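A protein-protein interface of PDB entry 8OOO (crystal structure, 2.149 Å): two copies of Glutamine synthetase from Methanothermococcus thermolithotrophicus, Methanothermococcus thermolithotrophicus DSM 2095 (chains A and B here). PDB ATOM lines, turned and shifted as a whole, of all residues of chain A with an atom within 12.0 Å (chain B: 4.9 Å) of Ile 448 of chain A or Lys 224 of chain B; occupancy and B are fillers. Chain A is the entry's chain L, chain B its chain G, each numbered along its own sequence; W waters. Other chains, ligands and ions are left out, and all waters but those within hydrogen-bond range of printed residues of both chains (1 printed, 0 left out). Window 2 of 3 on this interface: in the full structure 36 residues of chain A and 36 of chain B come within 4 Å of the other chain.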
ATOM      1  N   VAL A 437     -40.637  -6.004  20.918  1.00  0.00           N
ATOM      2  CA  VAL A 437     -39.617  -7.058  20.934  1.00  0.00           C
ATOM      3  C   VAL A 437     -40.070  -8.082  19.898  1.00  0.00           C
ATOM      4  O   VAL A 437     -41.120  -8.734  20.069  1.00  0.00           O
ATOM      5  CB  VAL A 437     -39.453  -7.697  22.326  1.00  0.00           C
ATOM      6  CG1 VAL A 437     -38.396  -8.795  22.283  1.00  0.00           C
ATOM      7  CG2 VAL A 437     -39.104  -6.630  23.377  1.00  0.00           C
ATOM      8  N   TRP A 440     -37.655 -12.176  15.712  1.00  0.00           N
ATOM      9  CA  TRP A 440     -36.291 -12.278  15.177  1.00  0.00           C
ATOM     10  C   TRP A 440     -35.292 -12.113  16.323  1.00  0.00           C
ATOM     11  O   TRP A 440     -34.355 -12.921  16.456  1.00  0.00           O
ATOM     12  CB  TRP A 440     -36.024 -11.225  14.077  1.00  0.00           C
ATOM     13  CG  TRP A 440     -34.644 -11.330  13.452  1.00  0.00           C
ATOM     14  CD1 TRP A 440     -34.319 -11.947  12.282  1.00  0.00           C
ATOM     15  CD2 TRP A 440     -33.409 -10.784  13.970  1.00  0.00           C
ATOM     16  NE1 TRP A 440     -32.972 -11.818  12.033  1.00  0.00           N
ATOM     17  CE2 TRP A 440     -32.379 -11.169  13.087  1.00  0.00           C
ATOM     18  CE3 TRP A 440     -33.072 -10.041  15.109  1.00  0.00           C
ATOM     19  CZ2 TRP A 440     -31.046 -10.772  13.274  1.00  0.00           C
ATOM     20  CZ3 TRP A 440     -31.749  -9.681  15.314  1.00  0.00           C
ATOM     21  CH2 TRP A 440     -30.745 -10.081  14.422  1.00  0.00           C
ATOM     22  N   GLU A 441     -35.560 -11.118  17.201  1.00  0.00           N
ATOM     23  CA  GLU A 441     -34.724 -10.817  18.358  1.00  0.00           C
ATOM     24  C   GLU A 441     -34.745 -11.944  19.388  1.00  0.00           C
ATOM     25  O   GLU A 441     -33.727 -12.237  19.975  1.00  0.00           O
ATOM     26  CB  GLU A 441     -35.180  -9.508  19.005  1.00  0.00           C
ATOM     27  CG  GLU A 441     -34.983  -8.279  18.134  1.00  0.00           C
ATOM     28  CD  GLU A 441     -35.776  -7.100  18.677  1.00  0.00           C
ATOM     29  OE1 GLU A 441     -36.844  -6.780  18.099  1.00  0.00           O
ATOM     30  OE2 GLU A 441     -35.366  -6.544  19.725  1.00  0.00           O
ATOM     31  N   THR A 442     -35.899 -12.553  19.657  1.00  0.00           N
ATOM     32  CA  THR A 442     -35.991 -13.653  20.608  1.00  0.00           C
ATOM     33  C   THR A 442     -35.165 -14.817  20.099  1.00  0.00           C
ATOM     34  O   THR A 442     -34.448 -15.426  20.875  1.00  0.00           O
ATOM     35  CB  THR A 442     -37.482 -14.047  20.834  1.00  0.00           C
ATOM     36  OG1 THR A 442     -38.133 -12.981  21.506  1.00  0.00           O
ATOM     37  CG2 THR A 442     -37.643 -15.355  21.667  1.00  0.00           C
ATOM     38  N   THR A 443     -35.277 -15.136  18.799  1.00  0.00           N
ATOM     39  CA  THR A 443     -34.519 -16.235  18.211  1.00  0.00           C
ATOM     40  C   THR A 443     -33.016 -15.923  18.292  1.00  0.00           C
ATOM     41  O   THR A 443     -32.209 -16.814  18.595  1.00  0.00           O
ATOM     42  CB  THR A 443     -34.926 -16.433  16.720  1.00  0.00           C
ATOM     43  OG1 THR A 443     -36.284 -16.832  16.611  1.00  0.00           O
ATOM     44  CG2 THR A 443     -34.048 -17.442  16.001  1.00  0.00           C
ATOM     45  N   ALA A 444     -32.638 -14.678  17.982  1.00  0.00           N
ATOM     46  CA  ALA A 444     -31.242 -14.300  17.914  1.00  0.00           C
ATOM     47  C   ALA A 444     -30.586 -14.178  19.255  1.00  0.00           C
ATOM     48  O   ALA A 444     -29.423 -14.551  19.406  1.00  0.00           O
ATOM     49  CB  ALA A 444     -31.111 -12.972  17.166  1.00  0.00           C
ATOM     50  N   TYR A 445     -31.298 -13.631  20.252  1.00  0.00           N
ATOM     51  CA  TYR A 445     -30.668 -13.212  21.512  1.00  0.00           C
ATOM     52  C   TYR A 445     -31.096 -13.888  22.801  1.00  0.00           C
ATOM     53  O   TYR A 445     -30.449 -13.634  23.836  1.00  0.00           O
ATOM     54  CB  TYR A 445     -30.886 -11.697  21.685  1.00  0.00           C
ATOM     55  CG  TYR A 445     -30.419 -10.893  20.494  1.00  0.00           C
ATOM     56  CD1 TYR A 445     -29.130 -11.039  19.991  1.00  0.00           C
ATOM     57  CD2 TYR A 445     -31.261  -9.990  19.867  1.00  0.00           C
ATOM     58  CE1 TYR A 445     -28.686 -10.287  18.908  1.00  0.00           C
ATOM     59  CE2 TYR A 445     -30.827  -9.230  18.779  1.00  0.00           C
ATOM     60  CZ  TYR A 445     -29.535  -9.373  18.310  1.00  0.00           C
ATOM     61  OH  TYR A 445     -29.086  -8.609  17.254  1.00  0.00           O
ATOM     62  N   LEU A 446     -32.143 -14.728  22.803  1.00  0.00           N
ATOM     63  CA  LEU A 446     -32.517 -15.341  24.084  1.00  0.00           C
ATOM     64  C   LEU A 446     -31.396 -16.176  24.688  1.00  0.00           C
ATOM     65  O   LEU A 446     -31.225 -16.162  25.908  1.00  0.00           O
ATOM     66  CB  LEU A 446     -33.825 -16.131  23.990  1.00  0.00           C
ATOM     67  CG  LEU A 446     -34.586 -16.291  25.306  1.00  0.00           C
ATOM     68  CD1 LEU A 446     -35.154 -14.965  25.802  1.00  0.00           C
ATOM     69  CD2 LEU A 446     -35.710 -17.281  25.143  1.00  0.00           C
ATOM     70  N   LYS A 447     -30.562 -16.787  23.817  1.00  0.00           N
ATOM     71  CA  LYS A 447     -29.450 -17.624  24.259  1.00  0.00           C
ATOM     72  C   LYS A 447     -28.279 -16.888  24.903  1.00  0.00           C
ATOM     73  O   LYS A 447     -27.408 -17.557  25.469  1.00  0.00           O
ATOM     74  CB  LYS A 447     -28.902 -18.420  23.079  1.00  0.00           C
ATOM     75  CG  LYS A 447     -28.105 -17.576  22.091  1.00  0.00           C
ATOM     76  CD  LYS A 447     -28.056 -18.248  20.743  1.00  0.00           C
ATOM     77  CE  LYS A 447     -27.364 -17.434  19.692  1.00  0.00           C
ATOM     78  NZ  LYS A 447     -27.855 -17.805  18.335  1.00  0.00           N
ATOM     79  N   ILE A 448     -28.211 -15.557  24.815  1.00  0.00           N
ATOM     80  CA  ILE A 448     -27.055 -14.865  25.370  1.00  0.00           C
ATOM     81  C   ILE A 448     -27.091 -14.736  26.930  1.00  0.00           C
ATOM     82  O   ILE A 448     -28.152 -15.033  27.549  1.00  0.00           O
ATOM     83  CB  ILE A 448     -26.788 -13.538  24.653  1.00  0.00           C
ATOM     84  CG1 ILE A 448     -27.730 -12.433  25.102  1.00  0.00           C
ATOM     85  CG2 ILE A 448     -26.817 -13.759  23.133  1.00  0.00           C
ATOM     86  CD1 ILE A 448     -27.514 -11.194  24.347  1.00  0.00           C
ATOM     87  OXT ILE A 448     -26.000 -14.491  27.536  1.00  0.00           O
ATOM     88  N   LYS B 220     -21.492 -14.724  33.846  1.00  0.00           N
ATOM     89  CA  LYS B 220     -22.560 -15.121  32.933  1.00  0.00           C
ATOM     90  C   LYS B 220     -22.627 -16.657  32.739  1.00  0.00           C
ATOM     91  O   LYS B 220     -23.737 -17.211  32.662  1.00  0.00           O
ATOM     92  CB  LYS B 220     -22.450 -14.378  31.605  1.00  0.00           C
ATOM     93  CG  LYS B 220     -22.759 -12.885  31.762  1.00  0.00           C
ATOM     94  CD  LYS B 220     -22.075 -12.065  30.738  1.00  0.00           C
ATOM     95  CE  LYS B 220     -22.697 -12.234  29.385  1.00  0.00           C
ATOM     96  NZ  LYS B 220     -21.974 -11.458  28.335  1.00  0.00           N
ATOM     97  N   THR B 221     -21.481 -17.347  32.710  1.00  0.00           N
ATOM     98  CA  THR B 221     -21.480 -18.811  32.565  1.00  0.00           C
ATOM     99  C   THR B 221     -22.023 -19.424  33.822  1.00  0.00           C
ATOM    100  O   THR B 221     -22.758 -20.415  33.763  1.00  0.00           O
ATOM    101  CB  THR B 221     -20.056 -19.372  32.301  1.00  0.00           C
ATOM    102  OG1 THR B 221     -19.568 -18.825  31.075  1.00  0.00           O
ATOM    103  CG2 THR B 221     -20.017 -20.910  32.228  1.00  0.00           C
ATOM    104  N   THR B 222     -21.586 -18.900  34.977  1.00  0.00           N
ATOM    105  CA  THR B 222     -22.063 -19.392  36.260  1.00  0.00           C
ATOM    106  C   THR B 222     -23.569 -19.236  36.366  1.00  0.00           C
ATOM    107  O   THR B 222     -24.241 -20.194  36.745  1.00  0.00           O
ATOM    108  CB  THR B 222     -21.390 -18.637  37.400  1.00  0.00           C
ATOM    109  OG1 THR B 222     -20.002 -18.848  37.253  1.00  0.00           O
ATOM    110  CG2 THR B 222     -21.834 -19.136  38.771  1.00  0.00           C
ATOM    111  N   ILE B 223     -24.116 -18.061  35.998  1.00  0.00           N
ATOM    112  CA  ILE B 223     -25.558 -17.871  36.167  1.00  0.00           C
ATOM    113  C   ILE B 223     -26.339 -18.865  35.337  1.00  0.00           C
ATOM    114  O   ILE B 223     -27.354 -19.385  35.786  1.00  0.00           O
ATOM    115  CB  ILE B 223     -26.025 -16.399  35.907  1.00  0.00           C
ATOM    116  CG1 ILE B 223     -25.810 -15.500  37.155  1.00  0.00           C
ATOM    117  CG2 ILE B 223     -27.536 -16.366  35.561  1.00  0.00           C
ATOM    118  CD1 ILE B 223     -24.572 -15.577  37.791  1.00  0.00           C
ATOM    119  N   LYS B 224     -25.897 -19.041  34.102  1.00  0.00           N
ATOM    120  CA  LYS B 224     -26.538 -19.885  33.121  1.00  0.00           C
ATOM    121  C   LYS B 224     -26.472 -21.363  33.484  1.00  0.00           C
ATOM    122  O   LYS B 224     -27.479 -22.055  33.333  1.00  0.00           O
ATOM    123  CB  LYS B 224     -25.942 -19.631  31.735  1.00  0.00           C
ATOM    124  CG  LYS B 224     -26.259 -18.251  31.177  1.00  0.00           C
ATOM    125  CD  LYS B 224     -25.515 -18.029  29.862  1.00  0.00           C
ATOM    126  CE  LYS B 224     -26.353 -17.312  28.842  1.00  0.00           C
ATOM    127  NZ  LYS B 224     -27.595 -18.046  28.461  1.00  0.00           N
ATOM    128  N   THR B 225     -25.326 -21.852  33.976  1.00  0.00           N
ATOM    129  CA  THR B 225     -25.205 -23.253  34.345  1.00  0.00           C
ATOM    130  C   THR B 225     -25.972 -23.542  35.612  1.00  0.00           C
ATOM    131  O   THR B 225     -26.679 -24.534  35.654  1.00  0.00           O
ATOM    132  CB  THR B 225     -23.734 -23.721  34.440  1.00  0.00           C
ATOM    133  OG1 THR B 225     -23.116 -23.072  35.557  1.00  0.00           O
ATOM    134  CG2 THR B 225     -22.967 -23.432  33.180  1.00  0.00           C
ATOM    135  N   ILE B 226     -25.871 -22.695  36.647  1.00  0.00           N
ATOM    136  CA  ILE B 226     -26.623 -22.907  37.896  1.00  0.00           C
ATOM    137  C   ILE B 226     -28.148 -22.870  37.624  1.00  0.00           C
ATOM    138  O   ILE B 226     -28.871 -23.687  38.177  1.00  0.00           O
ATOM    139  CB  ILE B 226     -26.218 -21.854  38.980  1.00  0.00           C
ATOM    140  CG1 ILE B 226     -24.704 -21.902  39.312  1.00  0.00           C
ATOM    141  CG2 ILE B 226     -27.020 -22.026  40.254  1.00  0.00           C
ATOM    142  CD1 ILE B 226     -24.158 -23.244  39.765  1.00  0.00           C
ATOM    143  N   ALA B 227     -28.648 -21.949  36.797  1.00  0.00           N
ATOM    144  CA  ALA B 227     -30.082 -21.896  36.473  1.00  0.00           C
ATOM    145  C   ALA B 227     -30.516 -23.229  35.813  1.00  0.00           C
ATOM    146  O   ALA B 227     -31.531 -23.806  36.180  1.00  0.00           O
ATOM    147  CB  ALA B 227     -30.369 -20.723  35.539  1.00  0.00           C
ATOM    148  N   GLU B 228     -29.683 -23.736  34.898  1.00  0.00           N
ATOM    149  CA  GLU B 228     -29.988 -25.030  34.235  1.00  0.00           C
ATOM    150  C   GLU B 228     -30.114 -26.124  35.300  1.00  0.00           C
ATOM    151  O   GLU B 228     -31.039 -26.947  35.178  1.00  0.00           O
ATOM    152  CB  GLU B 228     -28.933 -25.384  33.187  1.00  0.00           C
ATOM    153  CG  GLU B 228     -28.835 -24.384  32.049  1.00  0.00           C
ATOM    154  CD  GLU B 228     -30.064 -24.226  31.166  1.00  0.00           C
ATOM    155  OE1 GLU B 228     -30.204 -23.159  30.542  1.00  0.00           O
ATOM    156  OE2 GLU B 228     -30.873 -25.166  31.101  1.00  0.00           O
ATOM    157  N   LYS B 233     -33.894 -21.471  32.789  1.00  0.00           N
ATOM    158  CA  LYS B 233     -32.991 -20.960  31.801  1.00  0.00           C
ATOM    159  C   LYS B 233     -32.694 -19.499  32.155  1.00  0.00           C
ATOM    160  O   LYS B 233     -33.613 -18.763  32.461  1.00  0.00           O
ATOM    161  CB  LYS B 233     -33.647 -21.083  30.428  1.00  0.00           C
ATOM    162  CG  LYS B 233     -32.857 -20.460  29.288  1.00  0.00           C
ATOM    163  CD  LYS B 233     -33.436 -20.854  27.921  1.00  0.00           C
ATOM    164  CE  LYS B 233     -32.369 -21.164  26.891  1.00  0.00           C
ATOM    165  NZ  LYS B 233     -31.583 -19.959  26.518  1.00  0.00           N
ATOM    166  N   ALA B 234     -31.425 -19.088  32.189  1.00  0.00           N
ATOM    167  CA  ALA B 234     -31.121 -17.680  32.460  1.00  0.00           C
ATOM    168  C   ALA B 234     -30.800 -16.992  31.138  1.00  0.00           C
ATOM    169  O   ALA B 234     -30.124 -17.580  30.288  1.00  0.00           O
ATOM    170  CB  ALA B 234     -29.921 -17.551  33.401  1.00  0.00           C
ATOM    171  N   THR B 235     -31.221 -15.715  30.987  1.00  0.00           N
ATOM    172  CA  THR B 235     -30.872 -14.967  29.800  1.00  0.00           C
ATOM    173  C   THR B 235     -30.313 -13.596  30.190  1.00  0.00           C
ATOM    174  O   THR B 235     -30.832 -12.919  31.099  1.00  0.00           O
ATOM    175  CB  THR B 235     -32.070 -14.852  28.840  1.00  0.00           C
ATOM    176  OG1 THR B 235     -31.632 -14.195  27.639  1.00  0.00           O
ATOM    177  CG2 THR B 235     -33.233 -14.056  29.429  1.00  0.00           C
ATOM    178  N   PHE B 236     -29.270 -13.186  29.483  1.00  0.00           N
ATOM    179  CA  PHE B 236     -28.706 -11.855  29.605  1.00  0.00           C
ATOM    180  C   PHE B 236     -29.131 -10.977  28.376  1.00  0.00           C
ATOM    181  O   PHE B 236     -28.561  -9.900  28.155  1.00  0.00           O
ATOM    182  CB  PHE B 236     -27.171 -11.967  29.702  1.00  0.00           C
ATOM    183  CG  PHE B 236     -26.717 -12.512  31.040  1.00  0.00           C
ATOM    184  CD1 PHE B 236     -26.571 -11.676  32.132  1.00  0.00           C
ATOM    185  CD2 PHE B 236     -26.497 -13.867  31.215  1.00  0.00           C
ATOM    186  CE1 PHE B 236     -26.166 -12.179  33.372  1.00  0.00           C
ATOM    187  CE2 PHE B 236     -26.116 -14.373  32.457  1.00  0.00           C
ATOM    188  CZ  PHE B 236     -25.958 -13.524  33.534  1.00  0.00           C
ATOM    189  N   MET B 237     -30.182 -11.407  27.624  1.00  0.00           N
ATOM    190  CA  MET B 237     -30.801 -10.628  26.561  1.00  0.00           C
ATOM    191  C   MET B 237     -31.224  -9.265  27.123  1.00  0.00           C
ATOM    192  O   MET B 237     -31.875  -9.228  28.176  1.00  0.00           O
ATOM    193  CB  MET B 237     -32.045 -11.363  26.050  1.00  0.00           C
ATOM    194  CG  MET B 237     -32.731 -10.670  24.867  1.00  0.00           C
ATOM    195  SD  MET B 237     -33.951 -11.767  24.137  1.00  0.00           S
ATOM    196  CE  MET B 237     -34.712 -10.669  22.945  1.00  0.00           C
ATOM    197  N   PRO B 238     -30.822  -8.130  26.509  1.00  0.00           N
ATOM    198  CA  PRO B 238     -31.184  -6.806  27.088  1.00  0.00           C
ATOM    199  C   PRO B 238     -32.676  -6.551  27.319  1.00  0.00           C
ATOM    200  O   PRO B 238     -33.057  -5.928  28.316  1.00  0.00           O
ATOM    201  CB  PRO B 238     -30.644  -5.801  26.054  1.00  0.00           C
ATOM    202  CG  PRO B 238     -29.608  -6.550  25.305  1.00  0.00           C
ATOM    203  CD  PRO B 238     -30.013  -7.989  25.277  1.00  0.00           C
ATOM    204  N   THR B 297     -26.276  -5.154  20.210  1.00  0.00           N
ATOM    205  CA  THR B 297     -27.259  -5.994  19.540  1.00  0.00           C
ATOM    206  C   THR B 297     -28.436  -5.149  19.054  1.00  0.00           C
ATOM    207  O   THR B 297     -28.609  -4.005  19.467  1.00  0.00           O
ATOM    208  CB  THR B 297     -27.704  -7.125  20.495  1.00  0.00           C
ATOM    209  OG1 THR B 297     -28.503  -6.564  21.536  1.00  0.00           O
ATOM    210  CG2 THR B 297     -26.517  -7.911  21.075  1.00  0.00           C
ATOM    211  N   SER B 345     -25.165  -7.827  27.004  1.00  0.00           N
ATOM    212  CA  SER B 345     -24.844  -8.439  25.727  1.00  0.00           C
ATOM    213  C   SER B 345     -23.468  -7.941  25.206  1.00  0.00           C
ATOM    214  O   SER B 345     -22.965  -8.473  24.224  1.00  0.00           O
ATOM    215  CB  SER B 345     -25.938  -8.154  24.704  1.00  0.00           C
ATOM    216  OG  SER B 345     -25.845  -6.855  24.143  1.00  0.00           O
HETATM  217  O   HOH W   1     -23.974 -12.395  26.648  1.00  0.00           O
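No position is printed for both chains.
Of the 14 pairs that touch across the chains among the printed residues, none has its exchanged pair printed and touching as well.
The side-chain hydroxyl (OG1) of Thr 235 of chain B is in hydrogen-bond range of the backbone NH (N) of Met 237 of chain B (3.1 Å).
The backbone carbonyl oxygen (O) of Ala 234 of chain B is in hydrogen-bond range of the side-chain amino group (NZ) of Lys 224 of chain B (3.2 Å).
Glu 441 of chain A touches Met 237 of chain B (O to CE, 3.5 Å).
Met 237 of chain B touches Thr 442 of chain A (CE to N, 3.97 Å).
Tyr 445 of chain A touches Met 237 of chain B (O to CB, 3.6 Å).
Tyr 445 of chain A touches Thr 297 of chain B.
Leu 446 of chain A touches Lys 233 of chain B (O to NZ, 3.9 Å).
Lys 447 of chain A touches Lys 233 of chain B (CA to NZ, 3.9 Å).
Ile 448 of chain A touches Thr 235 of chain B (O to CA, 3.5 Å).
Met 237 of chain B touches Ile 448 of chain A (N to CG1, 3.7 Å).
Ser 345 of chain B touches Ile 448 of chain A (CB to CD1, 3.4 Å).
Hydrophobic or aromatic side chains of chain B that line the printed part of chain A: Phe 236 and Met 237.
Among the printed residues, no Asp or Glu carboxylate lies within 4 Å of a Lys or Arg side-chain nitrogen of the other chain.
The backbone carbonyl oxygen (O) of Leu 446 of chain A is in hydrogen-bond range of the side-chain hydroxyl (OG1) of Thr 235 of chain B.
The side-chain amino group of Lys 224 of chain B is in hydrogen-bond range of the backbone carbonyl oxygen of Lys 447 of chain A.
The side-chain amino group (NZ) of Lys 224 of chain B lies within salt-bridge range of the chain-end carboxylate (O) of Ile 448 of chain A (3.2 Å).
SD of Met 237 of chain B sits at hydrogen-bond distance from N of Leu 446 of chain A (3.7 Å).
The backbone NH (N) of Phe 236 of chain B is in hydrogen-bond range of the chain-end carboxylate (O) of Ile 448 of chain A (2.9 Å).
Water W1 lies within hydrogen-bond range of the side-chain amino group of Lys 220 of chain B (2.8 Å) and the chain-end carboxylate of Ile 448 of chain A (3.0 Å).
Ile 448 of chain A touches just these residues of chain B: Lys 224 (3.1 Å), Thr 235 (3.5 Å), Phe 236 (2.9 Å), Met 237 (3.7 Å) and Ser 345 (3.4 Å).
No residue of chain A comes within 4 Å of Lys 220 of chain B.
No residue of chain A comes within 4 Å of Thr 221 of chain B.
No residue of chain A comes within 4 Å of Thr 222 of chain B.
No residue of chain A comes within 4 Å of Ile 223 of chain B.
No residue of chain A comes within 4 Å of Thr 225 of chain B.
No residue of chain A comes within 4 Å of Ile 226 of chain B.
No residue of chain A comes within 4 Å of Ala 227 of chain B.
Glu 228 of chain B touches none of the printed residues of chain A.
Of chain A, only Leu 446 and Lys 447 come within 4 Å of Lys 233 of chain B.
Ala 234 of chain B touches none of the printed residues of chain A.
Of chain A, only Leu 446 (2.7 Å) and Ile 448 (3.5 Å) come within 4 Å of Thr 235 of chain B.
Of the printed residues of chain A, Phe 236 of chain B touches Ile 448 (2.9 Å).
Of chain A, only Ile 448 comes within 4 Å of Ser 345 of chain B.
Of the printed residues of chain B, Lys 447 of chain A touches Lys 224 and Lys 233.
Printed residues of chain B within 4 Å of Thr 442 of chain A: Met 237.
Thr 443 of chain A touches none of the printed residues of chain B.
The nearest residue of chain A that does not touch Lys 224 of chain B is Leu 446 of chain A (4.8 Å).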
